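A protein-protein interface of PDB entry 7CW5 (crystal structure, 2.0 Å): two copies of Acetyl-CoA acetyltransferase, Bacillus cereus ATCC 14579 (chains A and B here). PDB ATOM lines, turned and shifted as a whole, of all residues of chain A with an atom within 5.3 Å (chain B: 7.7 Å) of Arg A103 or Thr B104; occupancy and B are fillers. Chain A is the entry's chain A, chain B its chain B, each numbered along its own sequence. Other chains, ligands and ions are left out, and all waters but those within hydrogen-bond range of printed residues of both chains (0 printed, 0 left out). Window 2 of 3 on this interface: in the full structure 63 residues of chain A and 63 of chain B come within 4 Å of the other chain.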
ATOM      1  N   SER A   2     -10.930  -6.103  -4.949  1.00  0.00           N
ATOM      2  CA  SER A   2     -10.788  -5.002  -3.948  1.00  0.00           C
ATOM      3  C   SER A   2      -9.883  -3.895  -4.508  1.00  0.00           C
ATOM      4  O   SER A   2      -8.788  -3.654  -3.934  1.00  0.00           O
ATOM      5  CB  SER A   2     -10.293  -5.504  -2.604  1.00  0.00           C
ATOM      6  OG  SER A   2     -11.289  -6.281  -1.955  1.00  0.00           O
ATOM      7  N   LYS A   3     -10.340  -3.273  -5.599  1.00  0.00           N
ATOM      8  CA  LYS A   3      -9.975  -1.895  -6.025  1.00  0.00           C
ATOM      9  C   LYS A   3     -11.197  -1.228  -6.679  1.00  0.00           C
ATOM     10  O   LYS A   3     -11.964  -1.953  -7.375  1.00  0.00           O
ATOM     11  CB  LYS A   3      -8.800  -1.922  -7.000  1.00  0.00           C
ATOM     12  CG  LYS A   3      -7.992  -0.639  -7.012  1.00  0.00           C
ATOM     13  CD  LYS A   3      -7.139  -0.526  -5.794  1.00  0.00           C
ATOM     14  CE  LYS A   3      -5.974   0.420  -5.968  1.00  0.00           C
ATOM     15  NZ  LYS A   3      -5.269   0.568  -4.677  1.00  0.00           N
ATOM     16  N   THR A   4     -11.369   0.090  -6.486  1.00  0.00           N
ATOM     17  CA  THR A   4     -12.551   0.849  -6.965  1.00  0.00           C
ATOM     18  C   THR A   4     -12.120   1.845  -8.043  1.00  0.00           C
ATOM     19  O   THR A   4     -11.237   2.657  -7.786  1.00  0.00           O
ATOM     20  CB  THR A   4     -13.304   1.522  -5.812  1.00  0.00           C
ATOM     21  OG1 THR A   4     -13.598   0.528  -4.821  1.00  0.00           O
ATOM     22  CG2 THR A   4     -14.615   2.135  -6.246  1.00  0.00           C
ATOM     23  N   ALA A  98     -18.875   3.838  -0.544  1.00  0.00           N
ATOM     24  CA  ALA A  98     -19.033   3.103  -1.821  1.00  0.00           C
ATOM     25  C   ALA A  98     -17.762   2.284  -2.078  1.00  0.00           C
ATOM     26  O   ALA A  98     -17.877   1.109  -2.443  1.00  0.00           O
ATOM     27  CB  ALA A  98     -19.325   4.040  -2.960  1.00  0.00           C
ATOM     28  N   ASP A  99     -16.589   2.874  -1.900  1.00  0.00           N
ATOM     29  CA  ASP A  99     -15.291   2.188  -2.150  1.00  0.00           C
ATOM     30  C   ASP A  99     -15.224   0.935  -1.257  1.00  0.00           C
ATOM     31  O   ASP A  99     -14.839  -0.160  -1.720  1.00  0.00           O
ATOM     32  CB  ASP A  99     -14.142   3.136  -1.839  1.00  0.00           C
ATOM     33  CG  ASP A  99     -12.783   2.463  -1.835  1.00  0.00           C
ATOM     34  OD1 ASP A  99     -12.402   1.984  -2.907  1.00  0.00           O
ATOM     35  OD2 ASP A  99     -12.150   2.370  -0.728  1.00  0.00           O
ATOM     36  N   GLN A 100     -15.608   1.093   0.002  1.00  0.00           N
ATOM     37  CA  GLN A 100     -15.557   0.000   0.999  1.00  0.00           C
ATOM     38  C   GLN A 100     -16.507  -1.112   0.575  1.00  0.00           C
ATOM     39  O   GLN A 100     -16.077  -2.299   0.561  1.00  0.00           O
ATOM     40  CB  GLN A 100     -15.839   0.546   2.403  1.00  0.00           C
ATOM     41  CG  GLN A 100     -14.684   1.401   2.903  1.00  0.00           C
ATOM     42  CD  GLN A 100     -14.916   1.993   4.268  1.00  0.00           C
ATOM     43  OE1 GLN A 100     -15.960   2.600   4.536  1.00  0.00           O
ATOM     44  NE2 GLN A 100     -13.938   1.817   5.148  1.00  0.00           N
ATOM     45  N   ILE A 101     -17.750  -0.769   0.257  1.00  0.00           N
ATOM     46  CA  ILE A 101     -18.779  -1.781  -0.139  1.00  0.00           C
ATOM     47  C   ILE A 101     -18.306  -2.546  -1.385  1.00  0.00           C
ATOM     48  O   ILE A 101     -18.350  -3.807  -1.396  1.00  0.00           O
ATOM     49  CB  ILE A 101     -20.162  -1.119  -0.302  1.00  0.00           C
ATOM     50  CG1 ILE A 101     -20.667  -0.578   1.042  1.00  0.00           C
ATOM     51  CG2 ILE A 101     -21.139  -2.110  -0.922  1.00  0.00           C
ATOM     52  CD1 ILE A 101     -21.923   0.260   0.964  1.00  0.00           C
ATOM     53  N   ILE A 102     -17.805  -1.829  -2.383  1.00  0.00           N
ATOM     54  CA  ILE A 102     -17.291  -2.459  -3.622  1.00  0.00           C
ATOM     55  C   ILE A 102     -16.101  -3.380  -3.287  1.00  0.00           C
ATOM     56  O   ILE A 102     -16.046  -4.458  -3.869  1.00  0.00           O
ATOM     57  CB  ILE A 102     -16.944  -1.395  -4.679  1.00  0.00           C
ATOM     58  CG1 ILE A 102     -18.213  -0.888  -5.367  1.00  0.00           C
ATOM     59  CG2 ILE A 102     -15.909  -1.955  -5.660  1.00  0.00           C
ATOM     60  CD1 ILE A 102     -18.041   0.394  -6.153  1.00  0.00           C
ATOM     61  N   ARG A 103     -15.201  -2.982  -2.386  1.00  0.00           N
ATOM     62  CA  ARG A 103     -14.026  -3.787  -1.983  1.00  0.00           C
ATOM     63  C   ARG A 103     -14.466  -5.065  -1.236  1.00  0.00           C
ATOM     64  O   ARG A 103     -13.683  -6.042  -1.258  1.00  0.00           O
ATOM     65  CB  ARG A 103     -13.056  -2.926  -1.163  1.00  0.00           C
ATOM     66  CG  ARG A 103     -12.244  -1.974  -2.035  1.00  0.00           C
ATOM     67  CD  ARG A 103     -11.488  -0.918  -1.282  1.00  0.00           C
ATOM     68  NE  ARG A 103     -10.747  -1.492  -0.181  1.00  0.00           N
ATOM     69  CZ  ARG A 103     -10.702  -1.014   1.047  1.00  0.00           C
ATOM     70  NH1 ARG A 103     -10.025  -1.680   1.966  1.00  0.00           N
ATOM     71  NH2 ARG A 103     -11.331   0.104   1.369  1.00  0.00           N
ATOM     72  N   THR A 104     -15.681  -5.142  -0.685  1.00  0.00           N
ATOM     73  CA  THR A 104     -16.195  -6.421  -0.096  1.00  0.00           C
ATOM     74  C   THR A 104     -16.672  -7.376  -1.203  1.00  0.00           C
ATOM     75  O   THR A 104     -16.840  -8.563  -0.909  1.00  0.00           O
ATOM     76  CB  THR A 104     -17.379  -6.237   0.869  1.00  0.00           C
ATOM     77  OG1 THR A 104     -18.520  -5.791   0.127  1.00  0.00           O
ATOM     78  CG2 THR A 104     -17.076  -5.300   2.016  1.00  0.00           C
ATOM     79  N   GLY A 105     -16.944  -6.885  -2.415  1.00  0.00           N
ATOM     80  CA  GLY A 105     -17.622  -7.696  -3.443  1.00  0.00           C
ATOM     81  C   GLY A 105     -19.129  -7.745  -3.284  1.00  0.00           C
ATOM     82  O   GLY A 105     -19.788  -8.309  -4.196  1.00  0.00           O
ATOM     83  N   HIS A 279      -8.092   6.023   1.372  1.00  0.00           N
ATOM     84  CA  HIS A 279      -8.797   7.086   2.103  1.00  0.00           C
ATOM     85  C   HIS A 279      -8.575   6.841   3.584  1.00  0.00           C
ATOM     86  O   HIS A 279      -8.235   5.686   3.948  1.00  0.00           O
ATOM     87  CB  HIS A 279     -10.279   7.137   1.702  1.00  0.00           C
ATOM     88  CG  HIS A 279     -10.999   5.844   1.772  1.00  0.00           C
ATOM     89  ND1 HIS A 279     -11.490   5.334   2.966  1.00  0.00           N
ATOM     90  CD2 HIS A 279     -11.307   4.945   0.802  1.00  0.00           C
ATOM     91  CE1 HIS A 279     -12.071   4.181   2.726  1.00  0.00           C
ATOM     92  NE2 HIS A 279     -11.983   3.924   1.399  1.00  0.00           N
ATOM     93  N   THR B   4     -17.934 -11.290  10.686  1.00  0.00           N
ATOM     94  CA  THR B   4     -17.982 -10.262  11.755  1.00  0.00           C
ATOM     95  C   THR B   4     -18.681 -10.848  12.993  1.00  0.00           C
ATOM     96  O   THR B   4     -19.681 -11.536  12.841  1.00  0.00           O
ATOM     97  CB  THR B   4     -18.729  -9.016  11.289  1.00  0.00           C
ATOM     98  OG1 THR B   4     -18.093  -8.514  10.103  1.00  0.00           O
ATOM     99  CG2 THR B   4     -18.797  -7.960  12.364  1.00  0.00           C
ATOM    100  N   LEU B  97     -23.678  -2.103   7.505  1.00  0.00           N
ATOM    101  CA  LEU B  97     -22.554  -1.231   7.023  1.00  0.00           C
ATOM    102  C   LEU B  97     -21.311  -1.506   7.881  1.00  0.00           C
ATOM    103  O   LEU B  97     -20.218  -1.658   7.306  1.00  0.00           O
ATOM    104  CB  LEU B  97     -22.904   0.252   7.130  1.00  0.00           C
ATOM    105  CG  LEU B  97     -23.483   0.928   5.896  1.00  0.00           C
ATOM    106  CD1 LEU B  97     -24.045   2.300   6.275  1.00  0.00           C
ATOM    107  CD2 LEU B  97     -22.424   1.047   4.816  1.00  0.00           C
ATOM    108  N   ALA B  98     -21.476  -1.655   9.205  1.00  0.00           N
ATOM    109  CA  ALA B  98     -20.377  -2.012  10.125  1.00  0.00           C
ATOM    110  C   ALA B  98     -19.785  -3.354   9.686  1.00  0.00           C
ATOM    111  O   ALA B  98     -18.546  -3.480   9.587  1.00  0.00           O
ATOM    112  CB  ALA B  98     -20.853  -2.071  11.563  1.00  0.00           C
ATOM    113  N   ASP B  99     -20.648  -4.311   9.359  1.00  0.00           N
ATOM    114  CA  ASP B  99     -20.209  -5.642   8.888  1.00  0.00           C
ATOM    115  C   ASP B  99     -19.339  -5.460   7.625  1.00  0.00           C
ATOM    116  O   ASP B  99     -18.232  -6.034   7.568  1.00  0.00           O
ATOM    117  CB  ASP B  99     -21.391  -6.583   8.690  1.00  0.00           C
ATOM    118  CG  ASP B  99     -20.992  -7.883   8.011  1.00  0.00           C
ATOM    119  OD1 ASP B  99     -20.349  -8.716   8.692  1.00  0.00           O
ATOM    120  OD2 ASP B  99     -21.311  -8.038   6.801  1.00  0.00           O
ATOM    121  N   GLN B 100     -19.797  -4.701   6.634  1.00  0.00           N
ATOM    122  CA  GLN B 100     -19.031  -4.521   5.365  1.00  0.00           C
ATOM    123  C   GLN B 100     -17.683  -3.870   5.653  1.00  0.00           C
ATOM    124  O   GLN B 100     -16.673  -4.336   5.104  1.00  0.00           O
ATOM    125  CB  GLN B 100     -19.867  -3.773   4.332  1.00  0.00           C
ATOM    126  CG  GLN B 100     -21.115  -4.546   3.965  1.00  0.00           C
ATOM    127  CD  GLN B 100     -22.036  -3.724   3.101  1.00  0.00           C
ATOM    128  OE1 GLN B 100     -22.477  -2.634   3.462  1.00  0.00           O
ATOM    129  NE2 GLN B 100     -22.338  -4.260   1.937  1.00  0.00           N
ATOM    130  N   ILE B 101     -17.657  -2.810   6.453  1.00  0.00           N
ATOM    131  CA  ILE B 101     -16.394  -2.082   6.766  1.00  0.00           C
ATOM    132  C   ILE B 101     -15.395  -3.048   7.423  1.00  0.00           C
ATOM    133  O   ILE B 101     -14.196  -3.056   7.021  1.00  0.00           O
ATOM    134  CB  ILE B 101     -16.660  -0.819   7.599  1.00  0.00           C
ATOM    135  CG1 ILE B 101     -17.459   0.205   6.783  1.00  0.00           C
ATOM    136  CG2 ILE B 101     -15.343  -0.249   8.104  1.00  0.00           C
ATOM    137  CD1 ILE B 101     -18.114   1.299   7.576  1.00  0.00           C
ATOM    138  N   ILE B 102     -15.842  -3.820   8.413  1.00  0.00           N
ATOM    139  CA  ILE B 102     -14.938  -4.743   9.153  1.00  0.00           C
ATOM    140  C   ILE B 102     -14.424  -5.808   8.173  1.00  0.00           C
ATOM    141  O   ILE B 102     -13.228  -6.068   8.191  1.00  0.00           O
ATOM    142  CB  ILE B 102     -15.652  -5.329  10.382  1.00  0.00           C
ATOM    143  CG1 ILE B 102     -15.805  -4.277  11.479  1.00  0.00           C
ATOM    144  CG2 ILE B 102     -14.931  -6.575  10.855  1.00  0.00           C
ATOM    145  CD1 ILE B 102     -16.726  -4.687  12.602  1.00  0.00           C
ATOM    146  N   ARG B 103     -15.274  -6.291   7.270  1.00  0.00           N
ATOM    147  CA  ARG B 103     -14.908  -7.292   6.235  1.00  0.00           C
ATOM    148  C   ARG B 103     -13.868  -6.720   5.271  1.00  0.00           C
ATOM    149  O   ARG B 103     -13.070  -7.508   4.763  1.00  0.00           O
ATOM    150  CB  ARG B 103     -16.158  -7.803   5.516  1.00  0.00           C
ATOM    151  CG  ARG B 103     -16.897  -8.855   6.336  1.00  0.00           C
ATOM    152  CD  ARG B 103     -18.311  -9.094   5.894  1.00  0.00           C
ATOM    153  NE  ARG B 103     -18.288  -9.422   4.490  1.00  0.00           N
ATOM    154  CZ  ARG B 103     -19.157  -9.013   3.582  1.00  0.00           C
ATOM    155  NH1 ARG B 103     -18.977  -9.375   2.333  1.00  0.00           N
ATOM    156  NH2 ARG B 103     -20.183  -8.248   3.898  1.00  0.00           N
ATOM    157  N   THR B 104     -13.796  -5.408   5.052  1.00  0.00           N
ATOM    158  CA  THR B 104     -12.685  -4.832   4.225  1.00  0.00           C
ATOM    159  C   THR B 104     -11.351  -4.854   4.986  1.00  0.00           C
ATOM    160  O   THR B 104     -10.338  -4.609   4.364  1.00  0.00           O
ATOM    161  CB  THR B 104     -12.903  -3.365   3.838  1.00  0.00           C
ATOM    162  OG1 THR B 104     -12.805  -2.551   5.007  1.00  0.00           O
ATOM    163  CG2 THR B 104     -14.201  -3.122   3.097  1.00  0.00           C
ATOM    164  N   GLY B 105     -11.362  -4.965   6.313  1.00  0.00           N
ATOM    165  CA  GLY B 105     -10.141  -4.774   7.117  1.00  0.00           C
ATOM    166  C   GLY B 105      -9.871  -3.333   7.495  1.00  0.00           C
ATOM    167  O   GLY B 105      -8.888  -3.128   8.198  1.00  0.00           O
ATOM    168  N   ASP B 106     -10.668  -2.353   7.043  1.00  0.00           N
ATOM    169  CA  ASP B 106     -10.372  -0.918   7.301  1.00  0.00           C
ATOM    170  C   ASP B 106     -10.536  -0.653   8.785  1.00  0.00           C
ATOM    171  O   ASP B 106      -9.786   0.171   9.329  1.00  0.00           O
ATOM    172  CB  ASP B 106     -11.190   0.048   6.455  1.00  0.00           C
ATOM    173  CG  ASP B 106     -10.831   0.038   4.978  1.00  0.00           C
ATOM    174  OD1 ASP B 106      -9.895  -0.706   4.588  1.00  0.00           O
ATOM    175  OD2 ASP B 106     -11.560   0.683   4.217  1.00  0.00           O
ATOM    176  N   GLN B 107     -11.410  -1.397   9.448  1.00  0.00           N
ATOM    177  CA  GLN B 107     -11.597  -1.247  10.911  1.00  0.00           C
ATOM    178  C   GLN B 107     -11.872  -2.631  11.464  1.00  0.00           C
ATOM    179  O   GLN B 107     -12.352  -3.471  10.700  1.00  0.00           O
ATOM    180  CB  GLN B 107     -12.799  -0.361  11.265  1.00  0.00           C
ATOM    181  CG  GLN B 107     -12.849   0.984  10.577  1.00  0.00           C
ATOM    182  CD  GLN B 107     -11.732   1.916  10.965  1.00  0.00           C
ATOM    183  OE1 GLN B 107     -11.106   1.784  12.015  1.00  0.00           O
ATOM    184  NE2 GLN B 107     -11.446   2.854  10.078  1.00  0.00           N
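The guanidinium group (NH1) of Arg A103 is in salt-bridge range of the side-chain carboxylate (OD1) of Asp B106, 2.8 Å away.
NE2 of Gln A100 is in hydrogen-bond range of OD2 of Asp B106 (2.8 Å).
The backbone carbonyl oxygen (O) of Ile A101 lies within hydrogen-bond range of the side-chain hydroxyl (OG1) of Thr A104 (2.5 Å).
OD2 of Asp A99 lies within salt-bridge range of NH2 of Arg A103 (3.2 Å).
The side-chain carboxylate (OD2) of Asp A99 sits at hydrogen-bond distance from a ring nitrogen (NE2) of His A279, at 2.6 Å.
The backbone NH (N) of Asp B106 lies within hydrogen-bond range of the side-chain hydroxyl (OG1) of Thr B104 (3.0 Å).
The side-chain hydroxyl (OG) of Ser A2 lies within hydrogen-bond range of the backbone carbonyl oxygen (O) of Arg A103, 2.5 Å away.
OD2 of Asp B99 lies within salt-bridge range of NH2 of Arg B103, at 3.1 Å.
Among the printed residues, pairs that only touch across the chains: Thr A104 with Gln B100, Gln A100 with Thr B104, Gln A100 with Ile B101, Ile A101 with Gln B100, Thr A104 with Thr B104, Arg A103 with Thr B104, Thr A104 with Arg B103, His A279 with Asp B106 and Ile A101 with Leu B97.
Lys A3 touches none of the printed residues of chain B.
Printed residues of chain B within 4 Å of Gln A100: Ile B101 (3.6 Å), Thr B104 (3.3 Å) and Asp B106 (2.8 Å).
Printed residues of chain B within 4 Å of Arg A103: Thr B104 and Asp B106.
Of the printed residues of chain A, Leu B97 touches Ile A101 (3.96 Å).
Of the printed residues of chain A, Arg B103 touches Thr A104 (3.8 Å).
Of the printed residues of chain A, Thr B104 touches Gln A100, Arg A103 and Thr A104.
Gln B107 touches none of the printed residues of chain A.
The nearest printed residue of chain B that does not touch Thr A104 is Ile B101 (5.1 Å).
Printed residues of chain A that touch a printed residue of chain B: Gln A100, Ile A101, Arg A103, Thr A104 and His A279.
Printed residues of chain B that touch a printed residue of chain A: Leu B97, Gln B100, Ile B101, Arg B103, Thr B104 and Asp B106.
Among the printed residues, 11 pairs touch across the chains.
Among the printed residues, Asp or Glu carboxylates within 4 Å of a Lys or Arg side-chain nitrogen of the other chain: Arg A103 with Asp B106.
Gln A100 touches Ile B101, and with the chains exchanged Ile A101 touches Gln B100.
Gln A100 touches Thr B104, and with the chains exchanged Thr A104 touches Gln B100.
Arg A103 touches Thr B104, and with the chains exchanged Thr A104 touches Arg B103.
Thr A104 touches its own counterpart, Thr B104.
Positions printed for both chains: 4, 98, 99, 100, 101, 102, 103, 104 and 105.
Of the 11 pairs that touch across the chains among the printed residues, 7 have their exchanged pair printed and touching as well.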
